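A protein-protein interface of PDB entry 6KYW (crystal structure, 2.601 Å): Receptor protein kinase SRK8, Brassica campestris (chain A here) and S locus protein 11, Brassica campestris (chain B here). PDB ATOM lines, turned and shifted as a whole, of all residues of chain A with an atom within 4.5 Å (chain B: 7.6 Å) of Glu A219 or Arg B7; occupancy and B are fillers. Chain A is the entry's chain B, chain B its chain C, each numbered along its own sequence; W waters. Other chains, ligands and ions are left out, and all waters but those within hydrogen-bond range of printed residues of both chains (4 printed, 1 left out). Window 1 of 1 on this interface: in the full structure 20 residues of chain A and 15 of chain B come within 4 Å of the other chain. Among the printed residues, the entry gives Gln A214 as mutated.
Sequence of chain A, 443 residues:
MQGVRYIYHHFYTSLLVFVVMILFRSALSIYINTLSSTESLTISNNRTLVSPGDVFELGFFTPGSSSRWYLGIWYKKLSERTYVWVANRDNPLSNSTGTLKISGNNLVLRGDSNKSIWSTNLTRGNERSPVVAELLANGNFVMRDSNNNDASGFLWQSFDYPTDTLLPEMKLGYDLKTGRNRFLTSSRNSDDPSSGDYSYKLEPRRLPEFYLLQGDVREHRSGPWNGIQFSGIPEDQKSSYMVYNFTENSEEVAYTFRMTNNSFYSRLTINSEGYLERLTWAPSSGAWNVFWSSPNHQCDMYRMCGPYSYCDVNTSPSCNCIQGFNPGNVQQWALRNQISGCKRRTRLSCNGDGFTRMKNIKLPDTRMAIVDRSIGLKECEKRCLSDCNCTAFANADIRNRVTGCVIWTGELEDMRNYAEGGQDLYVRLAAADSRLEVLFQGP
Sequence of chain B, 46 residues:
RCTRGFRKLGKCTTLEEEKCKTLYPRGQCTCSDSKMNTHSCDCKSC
NH2 of Arg B7 is in hydrogen-bond range of O of Arg A218 (3.1 Å). The guanidinium group of Arg B7 sits at hydrogen-bond distance from the backbone carbonyl oxygen of Tyr A302 (2.9 Å). The side-chain hydroxyl (OG) of Ser B34 lies within hydrogen-bond range of the side-chain carboxylate (OE2) of Glu A219 (2.8 Å). The side-chain carboxylate of Glu A219 is in salt-bridge range of the side-chain amino group of Lys B35 (3.0 Å). NH2 of Arg A303 lies within salt-bridge range of OD1 of Asp B42.
O of Lys B35 sits at hydrogen-bond distance from OG1 of Thr B38 (3.1 Å). O of His B39 sits at hydrogen-bond distance from N of Lys B8 (2.9 Å). The side-chain hydroxyl (OG) of Ser B40 is in hydrogen-bond range of the side-chain carboxylate (OD2) of Asp B42 (2.6 Å). O of Leu A212 lies within hydrogen-bond range of N of Glu A219 (2.8 Å). NH1 of Arg B7 sits at hydrogen-bond distance from OG1 of Thr B38 (3.2 Å). N of Ser B32 sits at hydrogen-bond distance from O of Ser B40, 2.8 Å away.
Among the printed residues, merely in contact across the chains: Tyr A198 with Lys B35 (3.8 Å), Gln A214 with Asp B33 (3.8 Å), Val A217 with Ser B32 (3.5 Å), Val A217 with Ser B40 (3.5 Å), Val A217 with Asp B42 (3.4 Å), Glu A219 with Arg B7 (3.6 Å), Met A301 with Arg B7 (3.6 Å), Met A301 with Ser B34 (3.3 Å), Met A301 with Lys B35 (3.5 Å), Arg A303 with Gly B5 (3.2 Å), Arg A303 with Phe B6 (3.9 Å), Arg A303 with Arg B7 (3.5 Å), Met A304 with Arg B7 (3.98 Å), Met A304 with Lys B8 (3.9 Å), Met A304 with Leu B9 (3.7 Å), Met A304 with Thr B38 (3.7 Å), Ile A339 with Phe B6 (3.6 Å), Ile A339 with Arg B7 (3.7 Å) and Ile A339 with Lys B8 (3.8 Å).
Of chain B, only Arg B7 (3.6 Å), Ser B34 (2.8 Å) and Lys B35 (3.0 Å) come within 4 Å of Glu A219. Printed residues of chain A within 4 Å of Arg B7: Arg A218, Glu A219, Met A301, Tyr A302, Arg A303, Met A304 and Ile A339. Printed residues of chain B within 4 Å of Gln A214: Asp B33. Of the printed residues of chain A, Ser B32 touches Val A217 (3.5 Å). Of the printed residues of chain B, Tyr A198 touches Lys B35 (3.8 Å). Glu B16 touches none of the printed residues of chain A. The nearest residue of chain B that does not touch Glu A219 is Asp B33 (4.7 Å).
Of the 17 printed residues of chain B, 12 touch a printed residue of chain A. Hydrophobic or aromatic side chains of chain B that line the printed part of chain A: Phe B6 and Leu B9. Among the printed residues, 24 pairs touch across the chains. Among the printed residues, Asp or Glu carboxylates within 4 Å of a Lys or Arg side-chain nitrogen of the other chain: Glu A219 with Lys B35 (3.0 Å) and Arg A303 with Asp B42 (3.5 Å).
Water W4 bridges the backbone carbonyl oxygen of Arg A303 (2.6 Å) and the backbone NH of Arg B7 (3.2 Å). Water W1 lies within hydrogen-bond range of OD1 of Asp B42 (2.7 Å), O of Arg A218 (2.7 Å) and NH2 of Arg B7 (3.3 Å). Water W2 bridges the backbone carbonyl oxygen (O) of Met A304 (2.7 Å) and the backbone carbonyl oxygen (O) of Arg B7 (2.8 Å). Water W3 lies within hydrogen-bond range of the side-chain carboxylate (OD1) of Asp B42 and the backbone NH (N) of Arg A218.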
ATOM      1  N   TYR A 198      -4.756 -16.665  22.812  1.00  0.00           N
ATOM      2  CA  TYR A 198      -4.289 -15.316  23.086  1.00  0.00           C
ATOM      3  C   TYR A 198      -4.056 -15.127  24.572  1.00  0.00           C
ATOM      4  O   TYR A 198      -4.828 -15.614  25.411  1.00  0.00           O
ATOM      5  CB  TYR A 198      -5.282 -14.262  22.591  1.00  0.00           C
ATOM      6  CG  TYR A 198      -5.475 -14.251  21.106  1.00  0.00           C
ATOM      7  CD1 TYR A 198      -4.581 -13.595  20.270  1.00  0.00           C
ATOM      8  CD2 TYR A 198      -6.564 -14.899  20.528  1.00  0.00           C
ATOM      9  CE1 TYR A 198      -4.759 -13.580  18.898  1.00  0.00           C
ATOM     10  CE2 TYR A 198      -6.754 -14.894  19.157  1.00  0.00           C
ATOM     11  CZ  TYR A 198      -5.850 -14.231  18.345  1.00  0.00           C
ATOM     12  OH  TYR A 198      -6.041 -14.221  16.986  1.00  0.00           O
ATOM     13  N   LEU A 212       0.671  -8.621  24.109  1.00  0.00           N
ATOM     14  CA  LEU A 212      -0.428  -9.476  23.685  1.00  0.00           C
ATOM     15  C   LEU A 212       0.155 -10.515  22.750  1.00  0.00           C
ATOM     16  O   LEU A 212       0.712 -10.158  21.706  1.00  0.00           O
ATOM     17  CB  LEU A 212      -1.513  -8.672  22.980  1.00  0.00           C
ATOM     18  CG  LEU A 212      -2.885  -9.289  23.170  1.00  0.00           C
ATOM     19  CD1 LEU A 212      -3.928  -8.213  23.019  1.00  0.00           C
ATOM     20  CD2 LEU A 212      -3.105 -10.420  22.195  1.00  0.00           C
ATOM     21  N   GLN A 214      -0.241 -14.173  20.455  1.00  0.00           N
ATOM     22  CA  GLN A 214      -0.987 -15.253  19.820  1.00  0.00           C
ATOM     23  C   GLN A 214      -0.090 -16.488  19.834  1.00  0.00           C
ATOM     24  O   GLN A 214       0.825 -16.614  19.013  1.00  0.00           O
ATOM     25  CB  GLN A 214      -1.400 -14.879  18.399  1.00  0.00           C
ATOM     26  CG  GLN A 214      -2.376 -15.861  17.803  1.00  0.00           C
ATOM     27  CD  GLN A 214      -2.253 -15.967  16.305  1.00  0.00           C
ATOM     28  OE1 GLN A 214      -1.226 -16.427  15.783  1.00  0.00           O
ATOM     29  NE2 GLN A 214      -3.296 -15.520  15.594  1.00  0.00           N
ATOM     30  N   VAL A 217       3.704 -15.654  19.639  1.00  0.00           N
ATOM     31  CA  VAL A 217       3.966 -14.566  18.704  1.00  0.00           C
ATOM     32  C   VAL A 217       3.483 -13.252  19.315  1.00  0.00           C
ATOM     33  O   VAL A 217       2.339 -13.145  19.780  1.00  0.00           O
ATOM     34  CB  VAL A 217       3.287 -14.840  17.352  1.00  0.00           C
ATOM     35  CG1 VAL A 217       3.443 -13.643  16.405  1.00  0.00           C
ATOM     36  CG2 VAL A 217       3.867 -16.106  16.735  1.00  0.00           C
ATOM     37  N   ARG A 218       4.357 -12.256  19.350  1.00  0.00           N
ATOM     38  CA  ARG A 218       3.976 -10.949  19.876  1.00  0.00           C
ATOM     39  C   ARG A 218       3.172 -10.188  18.832  1.00  0.00           C
ATOM     40  O   ARG A 218       3.663  -9.915  17.732  1.00  0.00           O
ATOM     41  CB  ARG A 218       5.211 -10.154  20.286  1.00  0.00           C
ATOM     42  CG  ARG A 218       5.838 -10.692  21.520  1.00  0.00           C
ATOM     43  CD  ARG A 218       7.300 -10.400  21.541  1.00  0.00           C
ATOM     44  NE  ARG A 218       7.792 -10.439  22.907  1.00  0.00           N
ATOM     45  CZ  ARG A 218       8.939  -9.898  23.290  1.00  0.00           C
ATOM     46  NH1 ARG A 218       9.710  -9.276  22.394  1.00  0.00           N
ATOM     47  NH2 ARG A 218       9.309  -9.984  24.562  1.00  0.00           N
ATOM     48  N   GLU A 219       1.940  -9.851  19.170  1.00  0.00           N
ATOM     49  CA  GLU A 219       1.102  -9.094  18.255  1.00  0.00           C
ATOM     50  C   GLU A 219       1.050  -7.620  18.601  1.00  0.00           C
ATOM     51  O   GLU A 219       0.847  -6.789  17.716  1.00  0.00           O
ATOM     52  CB  GLU A 219      -0.311  -9.673  18.269  1.00  0.00           C
ATOM     53  CG  GLU A 219      -0.474 -10.997  17.516  1.00  0.00           C
ATOM     54  CD  GLU A 219      -1.946 -11.289  17.198  1.00  0.00           C
ATOM     55  OE1 GLU A 219      -2.832 -10.854  17.977  1.00  0.00           O
ATOM     56  OE2 GLU A 219      -2.221 -11.936  16.167  1.00  0.00           O
ATOM     57  N   HIS A 220       1.288  -7.278  19.860  1.00  0.00           N
ATOM     58  CA  HIS A 220       1.056  -5.924  20.323  1.00  0.00           C
ATOM     59  C   HIS A 220       1.766  -5.733  21.656  1.00  0.00           C
ATOM     60  O   HIS A 220       1.912  -6.677  22.443  1.00  0.00           O
ATOM     61  CB  HIS A 220      -0.447  -5.641  20.450  1.00  0.00           C
ATOM     62  CG  HIS A 220      -0.770  -4.443  21.277  1.00  0.00           C
ATOM     63  ND1 HIS A 220      -0.553  -3.158  20.832  1.00  0.00           N
ATOM     64  CD2 HIS A 220      -1.291  -4.331  22.525  1.00  0.00           C
ATOM     65  CE1 HIS A 220      -0.935  -2.302  21.765  1.00  0.00           C
ATOM     66  NE2 HIS A 220      -1.388  -2.988  22.803  1.00  0.00           N
ATOM     67  N   ASP A 300      -0.631  -0.001  16.016  1.00  0.00           N
ATOM     68  CA  ASP A 300      -0.471  -0.645  17.309  1.00  0.00           C
ATOM     69  C   ASP A 300       0.007  -2.069  17.173  1.00  0.00           C
ATOM     70  O   ASP A 300       0.213  -2.732  18.190  1.00  0.00           O
ATOM     71  CB  ASP A 300      -1.789  -0.690  18.097  1.00  0.00           C
ATOM     72  CG  ASP A 300      -2.284   0.669  18.504  1.00  0.00           C
ATOM     73  OD1 ASP A 300      -1.550   1.666  18.323  1.00  0.00           O
ATOM     74  OD2 ASP A 300      -3.430   0.735  19.003  1.00  0.00           O
ATOM     75  N   MET A 301       0.119  -2.581  15.954  1.00  0.00           N
ATOM     76  CA  MET A 301       0.577  -3.949  15.818  1.00  0.00           C
ATOM     77  C   MET A 301       2.090  -3.991  15.970  1.00  0.00           C
ATOM     78  O   MET A 301       2.809  -3.099  15.496  1.00  0.00           O
ATOM     79  CB  MET A 301       0.110  -4.540  14.485  1.00  0.00           C
ATOM     80  CG  MET A 301      -1.421  -4.682  14.388  1.00  0.00           C
ATOM     81  SD  MET A 301      -2.205  -5.626  15.656  1.00  0.00           S
ATOM     82  CE  MET A 301      -1.647  -7.219  15.158  1.00  0.00           C
ATOM     83  N   TYR A 302       2.560  -5.010  16.680  1.00  0.00           N
ATOM     84  CA  TYR A 302       3.960  -5.098  17.060  1.00  0.00           C
ATOM     85  C   TYR A 302       4.863  -4.970  15.842  1.00  0.00           C
ATOM     86  O   TYR A 302       4.834  -5.811  14.937  1.00  0.00           O
ATOM     87  CB  TYR A 302       4.237  -6.425  17.773  1.00  0.00           C
ATOM     88  CG  TYR A 302       5.603  -6.415  18.418  1.00  0.00           C
ATOM     89  CD1 TYR A 302       5.985  -5.354  19.252  1.00  0.00           C
ATOM     90  CD2 TYR A 302       6.524  -7.417  18.160  1.00  0.00           C
ATOM     91  CE1 TYR A 302       7.228  -5.306  19.817  1.00  0.00           C
ATOM     92  CE2 TYR A 302       7.781  -7.383  18.730  1.00  0.00           C
ATOM     93  CZ  TYR A 302       8.128  -6.334  19.559  1.00  0.00           C
ATOM     94  OH  TYR A 302       9.381  -6.300  20.129  1.00  0.00           O
ATOM     95  N   ARG A 303       5.673  -3.920  15.832  1.00  0.00           N
ATOM     96  CA  ARG A 303       6.635  -3.673  14.763  1.00  0.00           C
ATOM     97  C   ARG A 303       5.950  -3.582  13.405  1.00  0.00           C
ATOM     98  O   ARG A 303       6.481  -4.036  12.389  1.00  0.00           O
ATOM     99  CB  ARG A 303       7.733  -4.731  14.741  1.00  0.00           C
ATOM    100  CG  ARG A 303       8.509  -4.828  16.031  1.00  0.00           C
ATOM    101  CD  ARG A 303       9.665  -5.827  15.900  1.00  0.00           C
ATOM    102  NE  ARG A 303       9.181  -7.183  15.653  1.00  0.00           N
ATOM    103  CZ  ARG A 303       9.854  -8.285  15.957  1.00  0.00           C
ATOM    104  NH1 ARG A 303      11.051  -8.187  16.513  1.00  0.00           N
ATOM    105  NH2 ARG A 303       9.317  -9.473  15.718  1.00  0.00           N
ATOM    106  N   MET A 304       4.756  -2.977  13.381  1.00  0.00           N
ATOM    107  CA  MET A 304       4.192  -2.590  12.097  1.00  0.00           C
ATOM    108  C   MET A 304       5.249  -1.925  11.258  1.00  0.00           C
ATOM    109  O   MET A 304       5.184  -1.962  10.024  1.00  0.00           O
ATOM    110  CB  MET A 304       3.014  -1.624  12.244  1.00  0.00           C
ATOM    111  CG  MET A 304       2.191  -1.460  10.928  1.00  0.00           C
ATOM    112  SD  MET A 304       1.433  -3.039  10.371  1.00  0.00           S
ATOM    113  CE  MET A 304       2.372  -3.450   8.879  1.00  0.00           C
ATOM    114  N   ILE A 339       9.999  -3.152   6.218  1.00  0.00           N
ATOM    115  CA  ILE A 339      10.614  -3.906   7.311  1.00  0.00           C
ATOM    116  C   ILE A 339      12.065  -3.480   7.555  1.00  0.00           C
ATOM    117  O   ILE A 339      12.560  -3.583   8.680  1.00  0.00           O
ATOM    118  CB  ILE A 339      10.519  -5.417   7.049  1.00  0.00           C
ATOM    119  CG1 ILE A 339      11.382  -5.837   5.851  1.00  0.00           C
ATOM    120  CG2 ILE A 339       9.080  -5.840   6.859  1.00  0.00           C
ATOM    121  CD1 ILE A 339      11.428  -7.360   5.713  1.00  0.00           C
ATOM    122  N   GLY B   5      12.304 -10.444  14.023  1.00  0.00           N
ATOM    123  CA  GLY B   5      11.086 -10.639  13.267  1.00  0.00           C
ATOM    124  C   GLY B   5      10.636  -9.331  12.656  1.00  0.00           C
ATOM    125  O   GLY B   5      11.212  -8.270  12.908  1.00  0.00           O
ATOM    126  N   PHE B   6       9.588  -9.423  11.847  1.00  0.00           N
ATOM    127  CA  PHE B   6       9.003  -8.232  11.248  1.00  0.00           C
ATOM    128  C   PHE B   6       7.530  -8.492  10.987  1.00  0.00           C
ATOM    129  O   PHE B   6       7.051  -9.625  11.085  1.00  0.00           O
ATOM    130  CB  PHE B   6       9.721  -7.856   9.953  1.00  0.00           C
ATOM    131  CG  PHE B   6       9.783  -8.976   8.961  1.00  0.00           C
ATOM    132  CD1 PHE B   6       8.739  -9.195   8.072  1.00  0.00           C
ATOM    133  CD2 PHE B   6      10.871  -9.836   8.934  1.00  0.00           C
ATOM    134  CE1 PHE B   6       8.795 -10.242   7.151  1.00  0.00           C
ATOM    135  CE2 PHE B   6      10.933 -10.875   8.016  1.00  0.00           C
ATOM    136  CZ  PHE B   6       9.894 -11.077   7.116  1.00  0.00           C
ATOM    137  N   ARG B   7       6.823  -7.426  10.621  1.00  0.00           N
ATOM    138  CA  ARG B   7       5.405  -7.484  10.300  1.00  0.00           C
ATOM    139  C   ARG B   7       5.160  -6.785   8.972  1.00  0.00           C
ATOM    140  O   ARG B   7       5.868  -5.838   8.615  1.00  0.00           O
ATOM    141  CB  ARG B   7       4.564  -6.848  11.399  1.00  0.00           C
ATOM    142  CG  ARG B   7       3.066  -6.985  11.191  1.00  0.00           C
ATOM    143  CD  ARG B   7       2.330  -6.381  12.339  1.00  0.00           C
ATOM    144  NE  ARG B   7       2.650  -7.094  13.563  1.00  0.00           N
ATOM    145  CZ  ARG B   7       2.245  -8.332  13.840  1.00  0.00           C
ATOM    146  NH1 ARG B   7       1.478  -8.995  12.993  1.00  0.00           N
ATOM    147  NH2 ARG B   7       2.601  -8.904  14.974  1.00  0.00           N
ATOM    148  N   LYS B   8       4.153  -7.263   8.242  1.00  0.00           N
ATOM    149  CA  LYS B   8       3.819  -6.755   6.914  1.00  0.00           C
ATOM    150  C   LYS B   8       2.308  -6.717   6.702  1.00  0.00           C
ATOM    151  O   LYS B   8       1.538  -7.454   7.333  1.00  0.00           O
ATOM    152  CB  LYS B   8       4.429  -7.622   5.812  1.00  0.00           C
ATOM    153  CG  LYS B   8       5.835  -7.308   5.446  1.00  0.00           C
ATOM    154  CD  LYS B   8       6.238  -8.213   4.295  1.00  0.00           C
ATOM    155  CE  LYS B   8       7.736  -8.174   4.042  1.00  0.00           C
ATOM    156  NZ  LYS B   8       8.132  -9.194   3.034  1.00  0.00           N
ATOM    157  N   LEU B   9       1.898  -5.872   5.760  1.00  0.00           N
ATOM    158  CA  LEU B   9       0.523  -5.900   5.271  1.00  0.00           C
ATOM    159  C   LEU B   9       0.251  -7.179   4.487  1.00  0.00           C
ATOM    160  O   LEU B   9       1.092  -7.648   3.720  1.00  0.00           O
ATOM    161  CB  LEU B   9       0.253  -4.718   4.356  1.00  0.00           C
ATOM    162  CG  LEU B   9      -0.636  -3.606   4.881  1.00  0.00           C
ATOM    163  CD1 LEU B   9      -0.069  -3.042   6.154  1.00  0.00           C
ATOM    164  CD2 LEU B   9      -0.705  -2.552   3.777  1.00  0.00           C
ATOM    165  N   GLY B  10      -0.935  -7.726   4.661  1.00  0.00           N
ATOM    166  CA  GLY B  10      -1.343  -8.815   3.815  1.00  0.00           C
ATOM    167  C   GLY B  10      -1.231 -10.144   4.509  1.00  0.00           C
ATOM    168  O   GLY B  10      -0.904 -10.250   5.696  1.00  0.00           O
ATOM    169  N   GLU B  16       6.868 -15.936   1.606  1.00  0.00           N
ATOM    170  CA  GLU B  16       7.144 -15.248   2.855  1.00  0.00           C
ATOM    171  C   GLU B  16       7.573 -16.233   3.936  1.00  0.00           C
ATOM    172  O   GLU B  16       8.410 -15.900   4.779  1.00  0.00           O
ATOM    173  CB  GLU B  16       5.911 -14.452   3.274  1.00  0.00           C
ATOM    174  CG  GLU B  16       6.151 -13.398   4.336  1.00  0.00           C
ATOM    175  CD  GLU B  16       6.680 -12.078   3.788  1.00  0.00           C
ATOM    176  OE1 GLU B  16       6.938 -11.952   2.566  1.00  0.00           O
ATOM    177  OE2 GLU B  16       6.838 -11.156   4.607  1.00  0.00           O
ATOM    178  N   SER B  32       3.070 -16.088  10.659  1.00  0.00           N
ATOM    179  CA  SER B  32       1.798 -16.130  11.381  1.00  0.00           C
ATOM    180  C   SER B  32       0.876 -15.044  10.837  1.00  0.00           C
ATOM    181  O   SER B  32       1.214 -13.858  10.907  1.00  0.00           O
ATOM    182  CB  SER B  32       2.002 -15.918  12.885  1.00  0.00           C
ATOM    183  OG  SER B  32       2.816 -16.915  13.448  1.00  0.00           O
ATOM    184  N   ASP B  33      -0.280 -15.443  10.300  1.00  0.00           N
ATOM    185  CA  ASP B  33      -1.312 -14.485   9.914  1.00  0.00           C
ATOM    186  C   ASP B  33      -1.892 -13.840  11.169  1.00  0.00           C
ATOM    187  O   ASP B  33      -2.024 -14.483  12.211  1.00  0.00           O
ATOM    188  CB  ASP B  33      -2.449 -15.176   9.129  1.00  0.00           C
ATOM    189  CG  ASP B  33      -2.118 -15.408   7.652  1.00  0.00           C
ATOM    190  OD1 ASP B  33      -1.581 -14.504   6.963  1.00  0.00           O
ATOM    191  OD2 ASP B  33      -2.412 -16.520   7.180  1.00  0.00           O
ATOM    192  N   SER B  34      -2.291 -12.576  11.057  1.00  0.00           N
ATOM    193  CA  SER B  34      -2.656 -11.806  12.239  1.00  0.00           C
ATOM    194  C   SER B  34      -3.863 -10.924  11.924  1.00  0.00           C
ATOM    195  O   SER B  34      -4.423 -10.969  10.831  1.00  0.00           O
ATOM    196  CB  SER B  34      -1.456 -10.983  12.728  1.00  0.00           C
ATOM    197  OG  SER B  34      -1.797 -10.272  13.912  1.00  0.00           O
ATOM    198  N   LYS B  35      -4.247 -10.088  12.888  1.00  0.00           N
ATOM    199  CA  LYS B  35      -5.401  -9.215  12.738  1.00  0.00           C
ATOM    200  C   LYS B  35      -5.045  -7.959  11.954  1.00  0.00           C
ATOM    201  O   LYS B  35      -3.870  -7.606  11.789  1.00  0.00           O
ATOM    202  CB  LYS B  35      -5.963  -8.803  14.100  1.00  0.00           C
ATOM    203  CG  LYS B  35      -4.944  -8.360  15.106  1.00  0.00           C
ATOM    204  CD  LYS B  35      -5.616  -7.851  16.340  1.00  0.00           C
ATOM    205  CE  LYS B  35      -6.331  -8.953  17.184  1.00  0.00           C
ATOM    206  NZ  LYS B  35      -5.733 -10.324  17.237  1.00  0.00           N
ATOM    207  N   ASN B  37      -5.374  -7.455   8.822  1.00  0.00           N
ATOM    208  CA  ASN B  37      -4.709  -7.801   7.568  1.00  0.00           C
ATOM    209  C   ASN B  37      -3.191  -7.569   7.637  1.00  0.00           C
ATOM    210  O   ASN B  37      -2.590  -6.969   6.743  1.00  0.00           O
ATOM    211  CB  ASN B  37      -5.324  -7.039   6.392  1.00  0.00           C
ATOM    212  CG  ASN B  37      -4.901  -7.621   5.034  1.00  0.00           C
ATOM    213  OD1 ASN B  37      -4.820  -8.840   4.854  1.00  0.00           O
ATOM    214  ND2 ASN B  37      -4.618  -6.746   4.085  1.00  0.00           N
ATOM    215  N   THR B  38      -2.560  -8.079   8.696  1.00  0.00           N
ATOM    216  CA  THR B  38      -1.096  -8.140   8.767  1.00  0.00           C
ATOM    217  C   THR B  38      -0.659  -9.574   9.043  1.00  0.00           C
ATOM    218  O   THR B  38      -1.428 -10.389   9.562  1.00  0.00           O
ATOM    219  CB  THR B  38      -0.489  -7.209   9.849  1.00  0.00           C
ATOM    220  OG1 THR B  38      -0.816  -7.690  11.165  1.00  0.00           O
ATOM    221  CG2 THR B  38      -0.962  -5.782   9.685  1.00  0.00           C
ATOM    222  N   HIS B  39       0.595  -9.872   8.682  1.00  0.00           N
ATOM    223  CA  HIS B  39       1.257 -11.112   9.080  1.00  0.00           C
ATOM    224  C   HIS B  39       2.647 -10.793   9.634  1.00  0.00           C
ATOM    225  O   HIS B  39       3.193  -9.701   9.418  1.00  0.00           O
ATOM    226  CB  HIS B  39       1.355 -12.095   7.905  1.00  0.00           C
ATOM    227  CG  HIS B  39       2.245 -11.629   6.795  1.00  0.00           C
ATOM    228  ND1 HIS B  39       1.834 -10.727   5.837  1.00  0.00           N
ATOM    229  CD2 HIS B  39       3.526 -11.941   6.489  1.00  0.00           C
ATOM    230  CE1 HIS B  39       2.826 -10.498   4.994  1.00  0.00           C
ATOM    231  NE2 HIS B  39       3.861 -11.229   5.364  1.00  0.00           N
ATOM    232  N   SER B  40       3.225 -11.754  10.363  1.00  0.00           N
ATOM    233  CA  SER B  40       4.559 -11.586  10.930  1.00  0.00           C
ATOM    234  C   SER B  40       5.434 -12.817  10.717  1.00  0.00           C
ATOM    235  O   SER B  40       4.954 -13.955  10.670  1.00  0.00           O
ATOM    236  CB  SER B  40       4.496 -11.270  12.433  1.00  0.00           C
ATOM    237  OG  SER B  40       3.899 -12.331  13.167  1.00  0.00           O
ATOM    238  N   CYS B  41       6.739 -12.567  10.604  1.00  0.00           N
ATOM    239  CA  CYS B  41       7.775 -13.600  10.642  1.00  0.00           C
ATOM    240  C   CYS B  41       8.416 -13.618  12.029  1.00  0.00           C
ATOM    241  O   CYS B  41       8.984 -12.614  12.466  1.00  0.00           O
ATOM    242  CB  CYS B  41       8.831 -13.331   9.573  1.00  0.00           C
ATOM    243  SG  CYS B  41       8.401 -13.959   7.920  1.00  0.00           S
ATOM    244  N   ASP B  42       8.307 -14.738  12.732  1.00  0.00           N
ATOM    245  CA  ASP B  42       8.899 -14.851  14.061  1.00  0.00           C
ATOM    246  C   ASP B  42       9.543 -16.225  14.208  1.00  0.00           C
ATOM    247  O   ASP B  42       9.254 -17.158  13.454  1.00  0.00           O
ATOM    248  CB  ASP B  42       7.870 -14.651  15.181  1.00  0.00           C
ATOM    249  CG  ASP B  42       6.994 -13.436  14.952  1.00  0.00           C
ATOM    250  OD1 ASP B  42       7.295 -12.358  15.513  1.00  0.00           O
ATOM    251  OD2 ASP B  42       6.005 -13.556  14.194  1.00  0.00           O
HETATM  252  O   HOH W   1       5.490 -10.384  15.765  1.00  0.00           O
HETATM  253  O   HOH W   2       7.113  -3.281   8.642  1.00  0.00           O
HETATM  254  O   HOH W   3       6.989 -12.913  18.277  1.00  0.00           O
HETATM  255  O   HOH W   4       8.320  -4.569  10.557  1.00  0.00           O
